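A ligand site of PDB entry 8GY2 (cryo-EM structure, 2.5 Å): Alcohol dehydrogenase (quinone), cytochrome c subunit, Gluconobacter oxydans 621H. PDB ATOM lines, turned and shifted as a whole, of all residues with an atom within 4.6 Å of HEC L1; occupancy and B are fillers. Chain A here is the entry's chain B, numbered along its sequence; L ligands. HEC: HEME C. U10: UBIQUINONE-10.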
ATOM      1  N   SER A  54      12.182  27.020  16.773  1.00  0.00           N
ATOM      2  CA  SER A  54      11.735  25.954  15.877  1.00  0.00           C
ATOM      3  C   SER A  54      12.325  26.064  14.475  1.00  0.00           C
ATOM      4  O   SER A  54      11.991  25.236  13.622  1.00  0.00           O
ATOM      5  CB  SER A  54      10.214  25.934  15.808  1.00  0.00           C
ATOM      6  OG  SER A  54       9.636  26.195  17.070  1.00  0.00           O
ATOM      7  N   ASP A  55      13.167  27.062  14.220  1.00  0.00           N
ATOM      8  CA  ASP A  55      13.858  27.217  12.941  1.00  0.00           C
ATOM      9  C   ASP A  55      12.879  27.345  11.776  1.00  0.00           C
ATOM     10  O   ASP A  55      13.093  26.765  10.704  1.00  0.00           O
ATOM     11  CB  ASP A  55      14.846  26.073  12.697  1.00  0.00           C
ATOM     12  CG  ASP A  55      16.042  26.496  11.888  1.00  0.00           C
ATOM     13  OD1 ASP A  55      16.225  27.719  11.700  1.00  0.00           O
ATOM     14  OD2 ASP A  55      16.805  25.624  11.438  1.00  0.00           O
ATOM     15  N   CYS A  56      11.802  28.105  11.976  1.00  0.00           N
ATOM     16  CA  CYS A  56      10.818  28.275  10.909  1.00  0.00           C
ATOM     17  C   CYS A  56      11.378  29.113   9.767  1.00  0.00           C
ATOM     18  O   CYS A  56      11.111  28.829   8.597  1.00  0.00           O
ATOM     19  CB  CYS A  56       9.552  28.915  11.467  1.00  0.00           C
ATOM     20  SG  CYS A  56       8.835  28.054  12.883  1.00  0.00           S
ATOM     21  N   CYS A  59      13.941  27.479   6.625  1.00  0.00           N
ATOM     22  CA  CYS A  59      13.453  26.708   5.501  1.00  0.00           C
ATOM     23  C   CYS A  59      12.154  27.247   4.920  1.00  0.00           C
ATOM     24  O   CYS A  59      11.627  26.660   3.965  1.00  0.00           O
ATOM     25  CB  CYS A  59      13.272  25.239   5.912  1.00  0.00           C
ATOM     26  SG  CYS A  59      11.622  24.817   6.449  1.00  0.00           S
ATOM     27  N   HIS A  60      11.629  28.349   5.448  1.00  0.00           N
ATOM     28  CA  HIS A  60      10.444  28.994   4.888  1.00  0.00           C
ATOM     29  C   HIS A  60      10.784  30.305   4.192  1.00  0.00           C
ATOM     30  O   HIS A  60       9.895  31.135   3.956  1.00  0.00           O
ATOM     31  CB  HIS A  60       9.399  29.230   5.980  1.00  0.00           C
ATOM     32  CG  HIS A  60       8.364  28.150   6.060  1.00  0.00           C
ATOM     33  ND1 HIS A  60       7.382  27.987   5.110  1.00  0.00           N
ATOM     34  CD2 HIS A  60       8.148  27.192   6.993  1.00  0.00           C
ATOM     35  CE1 HIS A  60       6.623  26.961   5.441  1.00  0.00           C
ATOM     36  NE2 HIS A  60       7.060  26.468   6.580  1.00  0.00           N
ATOM     37  N   ILE A  74      13.094  22.387  -1.764  1.00  0.00           N
ATOM     38  CA  ILE A  74      13.469  21.285  -0.875  1.00  0.00           C
ATOM     39  C   ILE A  74      13.456  20.013  -1.700  1.00  0.00           C
ATOM     40  O   ILE A  74      12.421  19.632  -2.259  1.00  0.00           O
ATOM     41  CB  ILE A  74      12.517  21.179   0.329  1.00  0.00           C
ATOM     42  CG1 ILE A  74      12.830  22.274   1.348  1.00  0.00           C
ATOM     43  CG2 ILE A  74      12.640  19.805   0.980  1.00  0.00           C
ATOM     44  CD1 ILE A  74      11.656  22.636   2.227  1.00  0.00           C
ATOM     45  N   ILE A  81       9.824  19.958  -3.510  1.00  0.00           N
ATOM     46  CA  ILE A  81       8.757  20.662  -2.835  1.00  0.00           C
ATOM     47  C   ILE A  81       9.182  22.107  -2.642  1.00  0.00           C
ATOM     48  O   ILE A  81      10.369  22.458  -2.726  1.00  0.00           O
ATOM     49  CB  ILE A  81       8.390  20.003  -1.483  1.00  0.00           C
ATOM     50  CG1 ILE A  81       8.631  18.500  -1.542  1.00  0.00           C
ATOM     51  CG2 ILE A  81       6.933  20.285  -1.125  1.00  0.00           C
ATOM     52  CD1 ILE A  81       7.645  17.748  -2.410  1.00  0.00           C
ATOM     53  N   TYR A  82       8.204  22.971  -2.383  1.00  0.00           N
ATOM     54  CA  TYR A  82       8.461  24.382  -2.145  1.00  0.00           C
ATOM     55  C   TYR A  82       7.833  24.795  -0.823  1.00  0.00           C
ATOM     56  O   TYR A  82       6.706  24.399  -0.503  1.00  0.00           O
ATOM     57  CB  TYR A  82       7.902  25.240  -3.290  1.00  0.00           C
ATOM     58  CG  TYR A  82       8.575  24.988  -4.619  1.00  0.00           C
ATOM     59  CD1 TYR A  82       8.138  23.965  -5.446  1.00  0.00           C
ATOM     60  CD2 TYR A  82       9.647  25.751  -5.031  1.00  0.00           C
ATOM     61  CE1 TYR A  82       8.747  23.722  -6.658  1.00  0.00           C
ATOM     62  CE2 TYR A  82      10.275  25.519  -6.242  1.00  0.00           C
ATOM     63  CZ  TYR A  82       9.815  24.499  -7.051  1.00  0.00           C
ATOM     64  OH  TYR A  82      10.430  24.265  -8.263  1.00  0.00           O
ATOM     65  N   SER A  83       8.565  25.602  -0.060  1.00  0.00           N
ATOM     66  CA  SER A  83       8.055  26.080   1.214  1.00  0.00           C
ATOM     67  C   SER A  83       6.880  27.024   0.988  1.00  0.00           C
ATOM     68  O   SER A  83       6.956  27.944   0.161  1.00  0.00           O
ATOM     69  CB  SER A  83       9.163  26.788   1.999  1.00  0.00           C
ATOM     70  OG  SER A  83      10.389  26.089   1.903  1.00  0.00           O
ATOM     71  N   THR A  84       5.804  26.795   1.712  1.00  0.00           N
ATOM     72  CA  THR A  84       4.656  27.690   1.661  1.00  0.00           C
ATOM     73  C   THR A  84       4.964  28.985   2.409  1.00  0.00           C
ATOM     74  O   THR A  84       5.682  28.985   3.414  1.00  0.00           O
ATOM     75  CB  THR A  84       3.427  27.022   2.262  1.00  0.00           C
ATOM     76  OG1 THR A  84       3.308  25.681   1.756  1.00  0.00           O
ATOM     77  CG2 THR A  84       2.164  27.793   1.901  1.00  0.00           C
ATOM     78  N   ILE A  86       4.138  31.710   4.991  1.00  0.00           N
ATOM     79  CA  ILE A  86       3.388  31.700   6.230  1.00  0.00           C
ATOM     80  C   ILE A  86       3.198  33.121   6.777  1.00  0.00           C
ATOM     81  O   ILE A  86       2.979  33.302   7.970  1.00  0.00           O
ATOM     82  CB  ILE A  86       4.035  30.783   7.282  1.00  0.00           C
ATOM     83  CG1 ILE A  86       5.547  30.986   7.311  1.00  0.00           C
ATOM     84  CG2 ILE A  86       3.695  29.328   6.983  1.00  0.00           C
ATOM     85  CD1 ILE A  86       6.278  30.011   8.199  1.00  0.00           C
ATOM     86  N   ILE A  94      -1.122  32.571   5.543  1.00  0.00           N
ATOM     87  CA  ILE A  94      -1.996  31.908   6.501  1.00  0.00           C
ATOM     88  C   ILE A  94      -2.848  32.951   7.217  1.00  0.00           C
ATOM     89  O   ILE A  94      -3.231  32.761   8.373  1.00  0.00           O
ATOM     90  CB  ILE A  94      -1.183  31.074   7.505  1.00  0.00           C
ATOM     91  CG1 ILE A  94      -0.030  31.902   8.086  1.00  0.00           C
ATOM     92  CG2 ILE A  94      -0.655  29.812   6.845  1.00  0.00           C
ATOM     93  CD1 ILE A  94       0.743  31.202   9.172  1.00  0.00           C
ATOM     94  N   TYR A  97      -5.928  31.640   8.628  1.00  0.00           N
ATOM     95  CA  TYR A  97      -5.781  30.543   9.576  1.00  0.00           C
ATOM     96  C   TYR A  97      -6.215  30.987  10.966  1.00  0.00           C
ATOM     97  O   TYR A  97      -5.788  32.045  11.450  1.00  0.00           O
ATOM     98  CB  TYR A  97      -4.336  30.051   9.609  1.00  0.00           C
ATOM     99  CG  TYR A  97      -3.997  28.988   8.599  1.00  0.00           C
ATOM    100  CD1 TYR A  97      -4.220  29.194   7.244  1.00  0.00           C
ATOM    101  CD2 TYR A  97      -3.445  27.783   8.990  1.00  0.00           C
ATOM    102  CE1 TYR A  97      -3.911  28.223   6.308  1.00  0.00           C
ATOM    103  CE2 TYR A  97      -3.129  26.807   8.064  1.00  0.00           C
ATOM    104  CZ  TYR A  97      -3.363  27.034   6.728  1.00  0.00           C
ATOM    105  OH  TYR A  97      -3.047  26.058   5.812  1.00  0.00           O
ATOM    106  N   PHE A 102      -3.921  26.526  12.824  1.00  0.00           N
ATOM    107  CA  PHE A 102      -2.486  26.546  13.080  1.00  0.00           C
ATOM    108  C   PHE A 102      -2.058  25.312  13.878  1.00  0.00           C
ATOM    109  O   PHE A 102      -1.052  24.667  13.548  1.00  0.00           O
ATOM    110  CB  PHE A 102      -2.132  27.823  13.851  1.00  0.00           C
ATOM    111  CG  PHE A 102      -0.720  28.288  13.651  1.00  0.00           C
ATOM    112  CD1 PHE A 102      -0.216  28.504  12.379  1.00  0.00           C
ATOM    113  CD2 PHE A 102       0.095  28.526  14.748  1.00  0.00           C
ATOM    114  CE1 PHE A 102       1.084  28.947  12.215  1.00  0.00           C
ATOM    115  CE2 PHE A 102       1.390  28.960  14.575  1.00  0.00           C
ATOM    116  CZ  PHE A 102       1.888  29.168  13.314  1.00  0.00           C
ATOM    117  N   ALA A 105      -2.213  22.216  11.641  1.00  0.00           N
ATOM    118  CA  ALA A 105      -1.113  22.174  10.681  1.00  0.00           C
ATOM    119  C   ALA A 105       0.197  21.796  11.364  1.00  0.00           C
ATOM    120  O   ALA A 105       0.985  21.025  10.810  1.00  0.00           O
ATOM    121  CB  ALA A 105      -0.985  23.527   9.983  1.00  0.00           C
ATOM    122  N   LEU A 106       0.456  22.348  12.549  1.00  0.00           N
ATOM    123  CA  LEU A 106       1.730  22.077  13.214  1.00  0.00           C
ATOM    124  C   LEU A 106       1.790  20.671  13.814  1.00  0.00           C
ATOM    125  O   LEU A 106       2.799  19.981  13.677  1.00  0.00           O
ATOM    126  CB  LEU A 106       1.980  23.120  14.303  1.00  0.00           C
ATOM    127  CG  LEU A 106       2.473  24.467  13.773  1.00  0.00           C
ATOM    128  CD1 LEU A 106       2.313  25.536  14.831  1.00  0.00           C
ATOM    129  CD2 LEU A 106       3.925  24.353  13.335  1.00  0.00           C
ATOM    130  N   ARG A 111      -3.440  20.979   6.347  1.00  0.00           N
ATOM    131  CA  ARG A 111      -3.640  22.361   5.963  1.00  0.00           C
ATOM    132  C   ARG A 111      -5.074  22.793   6.214  1.00  0.00           C
ATOM    133  O   ARG A 111      -5.941  21.992   6.577  1.00  0.00           O
ATOM    134  CB  ARG A 111      -3.270  22.564   4.485  1.00  0.00           C
ATOM    135  CG  ARG A 111      -1.791  22.435   4.190  1.00  0.00           C
ATOM    136  CD  ARG A 111      -1.515  22.436   2.699  1.00  0.00           C
ATOM    137  NE  ARG A 111      -2.652  21.926   1.931  1.00  0.00           N
ATOM    138  CZ  ARG A 111      -2.711  21.909   0.606  1.00  0.00           C
ATOM    139  NH1 ARG A 111      -1.710  22.353  -0.133  1.00  0.00           N
ATOM    140  NH2 ARG A 111      -3.795  21.428   0.010  1.00  0.00           N
ATOM    141  N   VAL A 117       0.169  17.643   4.597  1.00  0.00           N
ATOM    142  CA  VAL A 117       1.420  18.168   4.066  1.00  0.00           C
ATOM    143  C   VAL A 117       2.437  17.044   3.912  1.00  0.00           C
ATOM    144  O   VAL A 117       2.293  15.948   4.486  1.00  0.00           O
ATOM    145  CB  VAL A 117       1.964  19.291   4.953  1.00  0.00           C
ATOM    146  CG1 VAL A 117       0.868  20.280   5.291  1.00  0.00           C
ATOM    147  CG2 VAL A 117       2.565  18.718   6.225  1.00  0.00           C
ATOM    148  N   TYR A 118       3.476  17.319   3.134  1.00  0.00           N
ATOM    149  CA  TYR A 118       4.551  16.359   2.975  1.00  0.00           C
ATOM    150  C   TYR A 118       5.355  16.252   4.271  1.00  0.00           C
ATOM    151  O   TYR A 118       5.398  17.195   5.064  1.00  0.00           O
ATOM    152  CB  TYR A 118       5.466  16.765   1.822  1.00  0.00           C
ATOM    153  CG  TYR A 118       4.906  16.428   0.461  1.00  0.00           C
ATOM    154  CD1 TYR A 118       4.945  15.130  -0.029  1.00  0.00           C
ATOM    155  CD2 TYR A 118       4.352  17.410  -0.339  1.00  0.00           C
ATOM    156  CE1 TYR A 118       4.440  14.819  -1.269  1.00  0.00           C
ATOM    157  CE2 TYR A 118       3.830  17.110  -1.590  1.00  0.00           C
ATOM    158  CZ  TYR A 118       3.889  15.811  -2.049  1.00  0.00           C
ATOM    159  OH  TYR A 118       3.376  15.506  -3.290  1.00  0.00           O
ATOM    160  N   ALA A 120       8.187  16.743   4.697  1.00  0.00           N
ATOM    161  CA  ALA A 120       9.158  17.832   4.754  1.00  0.00           C
ATOM    162  C   ALA A 120       8.849  18.773   5.902  1.00  0.00           C
ATOM    163  O   ALA A 120       9.767  19.349   6.505  1.00  0.00           O
ATOM    164  CB  ALA A 120       9.178  18.585   3.421  1.00  0.00           C
ATOM    165  N   MET A 121       7.573  18.961   6.214  1.00  0.00           N
ATOM    166  CA  MET A 121       7.198  19.625   7.454  1.00  0.00           C
ATOM    167  C   MET A 121       7.556  18.719   8.632  1.00  0.00           C
ATOM    168  O   MET A 121       7.127  17.556   8.664  1.00  0.00           O
ATOM    169  CB  MET A 121       5.712  19.931   7.479  1.00  0.00           C
ATOM    170  CG  MET A 121       5.365  21.403   7.424  1.00  0.00           C
ATOM    171  SD  MET A 121       5.832  22.280   8.923  1.00  0.00           S
ATOM    172  CE  MET A 121       4.454  21.885   9.993  1.00  0.00           C
ATOM    173  N   PRO A 122       8.315  19.205   9.603  1.00  0.00           N
ATOM    174  CA  PRO A 122       8.649  18.410  10.794  1.00  0.00           C
ATOM    175  C   PRO A 122       7.497  18.320  11.788  1.00  0.00           C
ATOM    176  O   PRO A 122       7.675  18.507  12.990  1.00  0.00           O
ATOM    177  CB  PRO A 122       9.851  19.148  11.382  1.00  0.00           C
ATOM    178  CG  PRO A 122      10.311  20.099  10.310  1.00  0.00           C
ATOM    179  CD  PRO A 122       9.079  20.460   9.552  1.00  0.00           C
ATOM    180  N   PHE A 126       6.954  18.606  15.617  1.00  0.00           N
ATOM    181  CA  PHE A 126       6.145  19.722  16.082  1.00  0.00           C
ATOM    182  C   PHE A 126       4.884  19.280  16.809  1.00  0.00           C
ATOM    183  O   PHE A 126       4.226  20.112  17.425  1.00  0.00           O
ATOM    184  CB  PHE A 126       5.778  20.634  14.913  1.00  0.00           C
ATOM    185  CG  PHE A 126       6.942  21.369  14.326  1.00  0.00           C
ATOM    186  CD1 PHE A 126       8.081  21.604  15.078  1.00  0.00           C
ATOM    187  CD2 PHE A 126       6.907  21.837  13.026  1.00  0.00           C
ATOM    188  CE1 PHE A 126       9.155  22.279  14.541  1.00  0.00           C
ATOM    189  CE2 PHE A 126       7.973  22.517  12.488  1.00  0.00           C
ATOM    190  CZ  PHE A 126       9.101  22.735  13.241  1.00  0.00           C
ATOM    191  N   MET A 137       3.352  31.441  19.054  1.00  0.00           N
ATOM    192  CA  MET A 137       3.769  31.449  17.650  1.00  0.00           C
ATOM    193  C   MET A 137       2.639  31.931  16.739  1.00  0.00           C
ATOM    194  O   MET A 137       2.892  32.625  15.752  1.00  0.00           O
ATOM    195  CB  MET A 137       4.249  30.069  17.235  1.00  0.00           C
ATOM    196  CG  MET A 137       5.749  29.878  17.365  1.00  0.00           C
ATOM    197  SD  MET A 137       6.374  28.396  16.561  1.00  0.00           S
ATOM    198  CE  MET A 137       4.928  27.343  16.630  1.00  0.00           C
ATOM    199  N   PHE A 141       2.951  35.088  14.279  1.00  0.00           N
ATOM    200  CA  PHE A 141       2.760  34.963  12.844  1.00  0.00           C
ATOM    201  C   PHE A 141       1.597  35.797  12.344  1.00  0.00           C
ATOM    202  O   PHE A 141       1.585  36.206  11.179  1.00  0.00           O
ATOM    203  CB  PHE A 141       2.572  33.493  12.462  1.00  0.00           C
ATOM    204  CG  PHE A 141       3.867  32.769  12.210  1.00  0.00           C
ATOM    205  CD1 PHE A 141       4.621  33.042  11.088  1.00  0.00           C
ATOM    206  CD2 PHE A 141       4.325  31.816  13.105  1.00  0.00           C
ATOM    207  CE1 PHE A 141       5.801  32.382  10.857  1.00  0.00           C
ATOM    208  CE2 PHE A 141       5.513  31.151  12.874  1.00  0.00           C
ATOM    209  CZ  PHE A 141       6.251  31.434  11.751  1.00  0.00           C
ATOM    210  N   ARG A 164      -2.220  13.743  -3.104  1.00  0.00           N
ATOM    211  CA  ARG A 164      -2.023  14.112  -1.712  1.00  0.00           C
ATOM    212  C   ARG A 164      -2.699  13.167  -0.730  1.00  0.00           C
ATOM    213  O   ARG A 164      -2.382  13.217   0.465  1.00  0.00           O
ATOM    214  CB  ARG A 164      -2.530  15.541  -1.471  1.00  0.00           C
ATOM    215  CG  ARG A 164      -1.676  16.357  -0.522  1.00  0.00           C
ATOM    216  CD  ARG A 164      -0.788  17.325  -1.285  1.00  0.00           C
ATOM    217  NE  ARG A 164      -0.348  18.430  -0.441  1.00  0.00           N
ATOM    218  CZ  ARG A 164       0.531  19.342  -0.800  1.00  0.00           C
ATOM    219  NH1 ARG A 164       1.124  19.301  -1.983  1.00  0.00           N
ATOM    220  NH2 ARG A 164       0.837  20.331   0.043  1.00  0.00           N
ATOM    221  N   HIS A 203      14.254  20.186  15.912  1.00  0.00           N
ATOM    222  CA  HIS A 203      14.034  18.851  15.371  1.00  0.00           C
ATOM    223  C   HIS A 203      15.375  18.319  14.901  1.00  0.00           C
ATOM    224  O   HIS A 203      15.705  18.388  13.719  1.00  0.00           O
ATOM    225  CB  HIS A 203      13.001  18.884  14.249  1.00  0.00           C
ATOM    226  CG  HIS A 203      13.116  20.099  13.367  1.00  0.00           C
ATOM    227  ND1 HIS A 203      12.644  21.341  13.750  1.00  0.00           N
ATOM    228  CD2 HIS A 203      13.644  20.265  12.140  1.00  0.00           C
ATOM    229  CE1 HIS A 203      12.887  22.209  12.793  1.00  0.00           C
ATOM    230  NE2 HIS A 203      13.493  21.580  11.802  1.00  0.00           N
HETATM  231 FE   HEC L   1       6.361  24.778   7.661  1.00  0.00          FE
HETATM  232  CHA HEC L   1       3.918  23.991   5.374  1.00  0.00           C
HETATM  233  CHB HEC L   1       4.118  26.624   9.413  1.00  0.00           C
HETATM  234  CHC HEC L   1       8.607  24.996  10.229  1.00  0.00           C
HETATM  235  CHD HEC L   1       8.729  23.499   5.644  1.00  0.00           C
HETATM  236  NA  HEC L   1       4.412  25.221   7.436  1.00  0.00           N
HETATM  237  C1A HEC L   1       3.559  24.808   6.436  1.00  0.00           C
HETATM  238  C2A HEC L   1       2.243  25.366   6.666  1.00  0.00           C
HETATM  239  C3A HEC L   1       2.307  26.089   7.793  1.00  0.00           C
HETATM  240  C4A HEC L   1       3.655  26.004   8.282  1.00  0.00           C
HETATM  241  CMA HEC L   1       1.182  26.891   8.490  1.00  0.00           C
HETATM  242  CAA HEC L   1       1.037  25.098   5.742  1.00  0.00           C
HETATM  243  CBA HEC L   1       0.696  26.285   4.821  1.00  0.00           C
HETATM  244  CGA HEC L   1      -0.074  25.860   3.585  1.00  0.00           C
HETATM  245  O1A HEC L   1       0.521  25.042   2.834  1.00  0.00           O
HETATM  246  O2A HEC L   1      -1.096  26.538   3.341  1.00  0.00           O
HETATM  247  NB  HEC L   1       6.365  25.639   9.459  1.00  0.00           N
HETATM  248  C1B HEC L   1       5.325  26.371  10.014  1.00  0.00           C
HETATM  249  C2B HEC L   1       5.726  26.821  11.301  1.00  0.00           C
HETATM  250  C3B HEC L   1       6.967  26.370  11.523  1.00  0.00           C
HETATM  251  C4B HEC L   1       7.387  25.620  10.380  1.00  0.00           C
HETATM  252  CMB HEC L   1       4.812  27.683  12.215  1.00  0.00           C
HETATM  253  CAB HEC L   1       7.792  26.630  12.821  1.00  0.00           C
HETATM  254  CBB HEC L   1       7.312  25.810  13.855  1.00  0.00           C
HETATM  255  NC  HEC L   1       8.288  24.336   7.884  1.00  0.00           N
HETATM  256  C1C HEC L   1       9.048  24.492   9.024  1.00  0.00           C
HETATM  257  C2C HEC L   1      10.410  24.059   8.779  1.00  0.00           C
HETATM  258  C3C HEC L   1      10.436  23.644   7.509  1.00  0.00           C
HETATM  259  C4C HEC L   1       9.141  23.799   6.920  1.00  0.00           C
HETATM  260  CMC HEC L   1      11.544  24.102   9.842  1.00  0.00           C
HETATM  261  CAC HEC L   1      11.702  23.070   6.747  1.00  0.00           C
HETATM  262  CBC HEC L   1      11.970  21.760   7.010  1.00  0.00           C
HETATM  263  ND  HEC L   1       6.322  23.915   5.850  1.00  0.00           N
HETATM  264  C1D HEC L   1       7.438  23.453   5.175  1.00  0.00           C
HETATM  265  C2D HEC L   1       7.000  22.908   3.901  1.00  0.00           C
HETATM  266  C3D HEC L   1       5.685  23.041   3.823  1.00  0.00           C
HETATM  267  C4D HEC L   1       5.235  23.681   5.051  1.00  0.00           C
HETATM  268  CMD HEC L   1       8.005  22.306   2.887  1.00  0.00           C
HETATM  269  CAD HEC L   1       4.736  22.626   2.678  1.00  0.00           C
HETATM  270  CBD HEC L   1       4.568  21.144   2.388  1.00  0.00           C
HETATM  271  CGD HEC L   1       3.578  20.842   1.316  1.00  0.00           C
HETATM  272  O1D HEC L   1       2.798  19.887   1.592  1.00  0.00           O
HETATM  273  O2D HEC L   1       3.428  21.679   0.392  1.00  0.00           O
HETATM  274  C1  U10 L   2       8.542  10.006   0.342  1.00  0.00           C
HETATM  275  C2  U10 L   2       7.985   8.745   0.283  1.00  0.00           C
HETATM  276  C3  U10 L   2       6.670   8.533   0.705  1.00  0.00           C
HETATM  277  C4  U10 L   2       5.925   9.620   1.183  1.00  0.00           C
HETATM  278  C5  U10 L   2       6.495  10.884   1.242  1.00  0.00           C
HETATM  279  C6  U10 L   2       7.805  11.088   0.821  1.00  0.00           C
HETATM  280  C1M U10 L   2       9.956  10.202  -0.114  1.00  0.00           C
HETATM  281  C3M U10 L   2       5.854   6.496   0.034  1.00  0.00           C
HETATM  282  C4M U10 L   2       3.699   9.038   1.372  1.00  0.00           C
HETATM  283  C7  U10 L   2       8.470  12.416   1.102  1.00  0.00           C
HETATM  284  C8  U10 L   2       9.179  12.407   2.438  1.00  0.00           C
HETATM  285  C9  U10 L   2      10.483  13.080   2.573  1.00  0.00           C
HETATM  286  C10 U10 L   2      10.859  14.172   1.610  1.00  0.00           C
HETATM  287  C11 U10 L   2      11.447  12.697   3.671  1.00  0.00           C
HETATM  288  C12 U10 L   2      11.452  13.767   4.757  1.00  0.00           C
HETATM  289  C13 U10 L   2      12.870  14.029   5.230  1.00  0.00           C
HETATM  290  C14 U10 L   2      13.194  15.300   5.888  1.00  0.00           C
HETATM  291  C15 U10 L   2      12.125  16.329   6.074  1.00  0.00           C
HETATM  292  C16 U10 L   2      14.587  15.568   6.420  1.00  0.00           C
HETATM  293  C17 U10 L   2      15.476  16.304   5.409  1.00  0.00           C
HETATM  294  C18 U10 L   2      15.105  17.767   5.294  1.00  0.00           C
HETATM  295  C19 U10 L   2      15.854  18.800   6.015  1.00  0.00           C
HETATM  296  C20 U10 L   2      15.813  18.850   7.514  1.00  0.00           C
HETATM  297  C21 U10 L   2      16.663  19.832   5.256  1.00  0.00           C
HETATM  298  C22 U10 L   2      15.783  21.036   4.940  1.00  0.00           C
HETATM  299  C23 U10 L   2      16.515  22.309   5.287  1.00  0.00           C
HETATM  300  C24 U10 L   2      16.525  23.447   4.344  1.00  0.00           C
HETATM  301  C25 U10 L   2      16.407  23.191   2.878  1.00  0.00           C
HETATM  302  C26 U10 L   2      16.659  24.850   4.867  1.00  0.00           C
HETATM  303  C27 U10 L   2      18.099  25.334   4.767  1.00  0.00           C
HETATM  304  C28 U10 L   2      18.196  26.365   3.664  1.00  0.00           C
HETATM  305  C29 U10 L   2      19.269  27.362   3.650  1.00  0.00           C
HETATM  306  O2  U10 L   2       8.722   7.778   0.128  1.00  0.00           O
HETATM  307  O3  U10 L   2       6.336   7.386   1.011  1.00  0.00           O
HETATM  308  O4  U10 L   2       4.946   9.413   1.911  1.00  0.00           O
HETATM  309  O5  U10 L   2       5.747  11.857   1.296  1.00  0.00           O
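The side-chain hydroxyl (OG) of Ser 83 is in hydrogen-bond range of the backbone carbonyl oxygen (O) of Cys 59, 2.5 Å away. A ring nitrogen (ND1) of His 60 is in hydrogen-bond range of the backbone carbonyl oxygen (O) of Thr 84, 2.6 Å away. The backbone NH (N) of Ile 74 lies within hydrogen-bond range of the backbone carbonyl oxygen (O) of Ile 81.
The side-chain sulfur (SD) of Met 121 lies close to a nitrogen (NC) of HEC L1, 3.4 Å away. Residues that only touch HEC L1: Ser 54 (3.5 Å), Asp 55 (3.2 Å), Ile 74 (3.7 Å), Ile 86 (3.6 Å), Ile 94 (3.8 Å), Phe 102 (3.5 Å), Leu 106 (3.6 Å), Arg 111 (3.3 Å), Val 117 (3.3 Å), Ala 120 (3.3 Å), Pro 122 (3.9 Å), Phe 126 (3.4 Å), Met 137 (3.9 Å), Phe 141 (3.6 Å) and His 203 (3.7 Å). Of the 27 residues printed, 23 come within 4 Å of HEC L1.
CAB of HEC L1 is covalently linked to SG of Cys 56 (1.8 Å). The side-chain sulfur of Cys 59 is bonded to a carbon (CAC) of HEC L1 (1.8 Å). A ring nitrogen (NE2) of His 60 binds an iron atom (FE) of HEC L1, 2.1 Å away. An oxygen (O1D) of HEC L1 lies within salt-bridge range of the guanidinium group of Arg 164. The side-chain hydroxyl (OG1) of Thr 84 is in hydrogen-bond range of an oxygen (O1A) of HEC L1, at 3.1 Å. O1D of HEC L1 sits at hydrogen-bond distance from N of Tyr 118 (3.1 Å). OH of Tyr 97 sits at hydrogen-bond distance from O2A of HEC L1 (3.2 Å).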
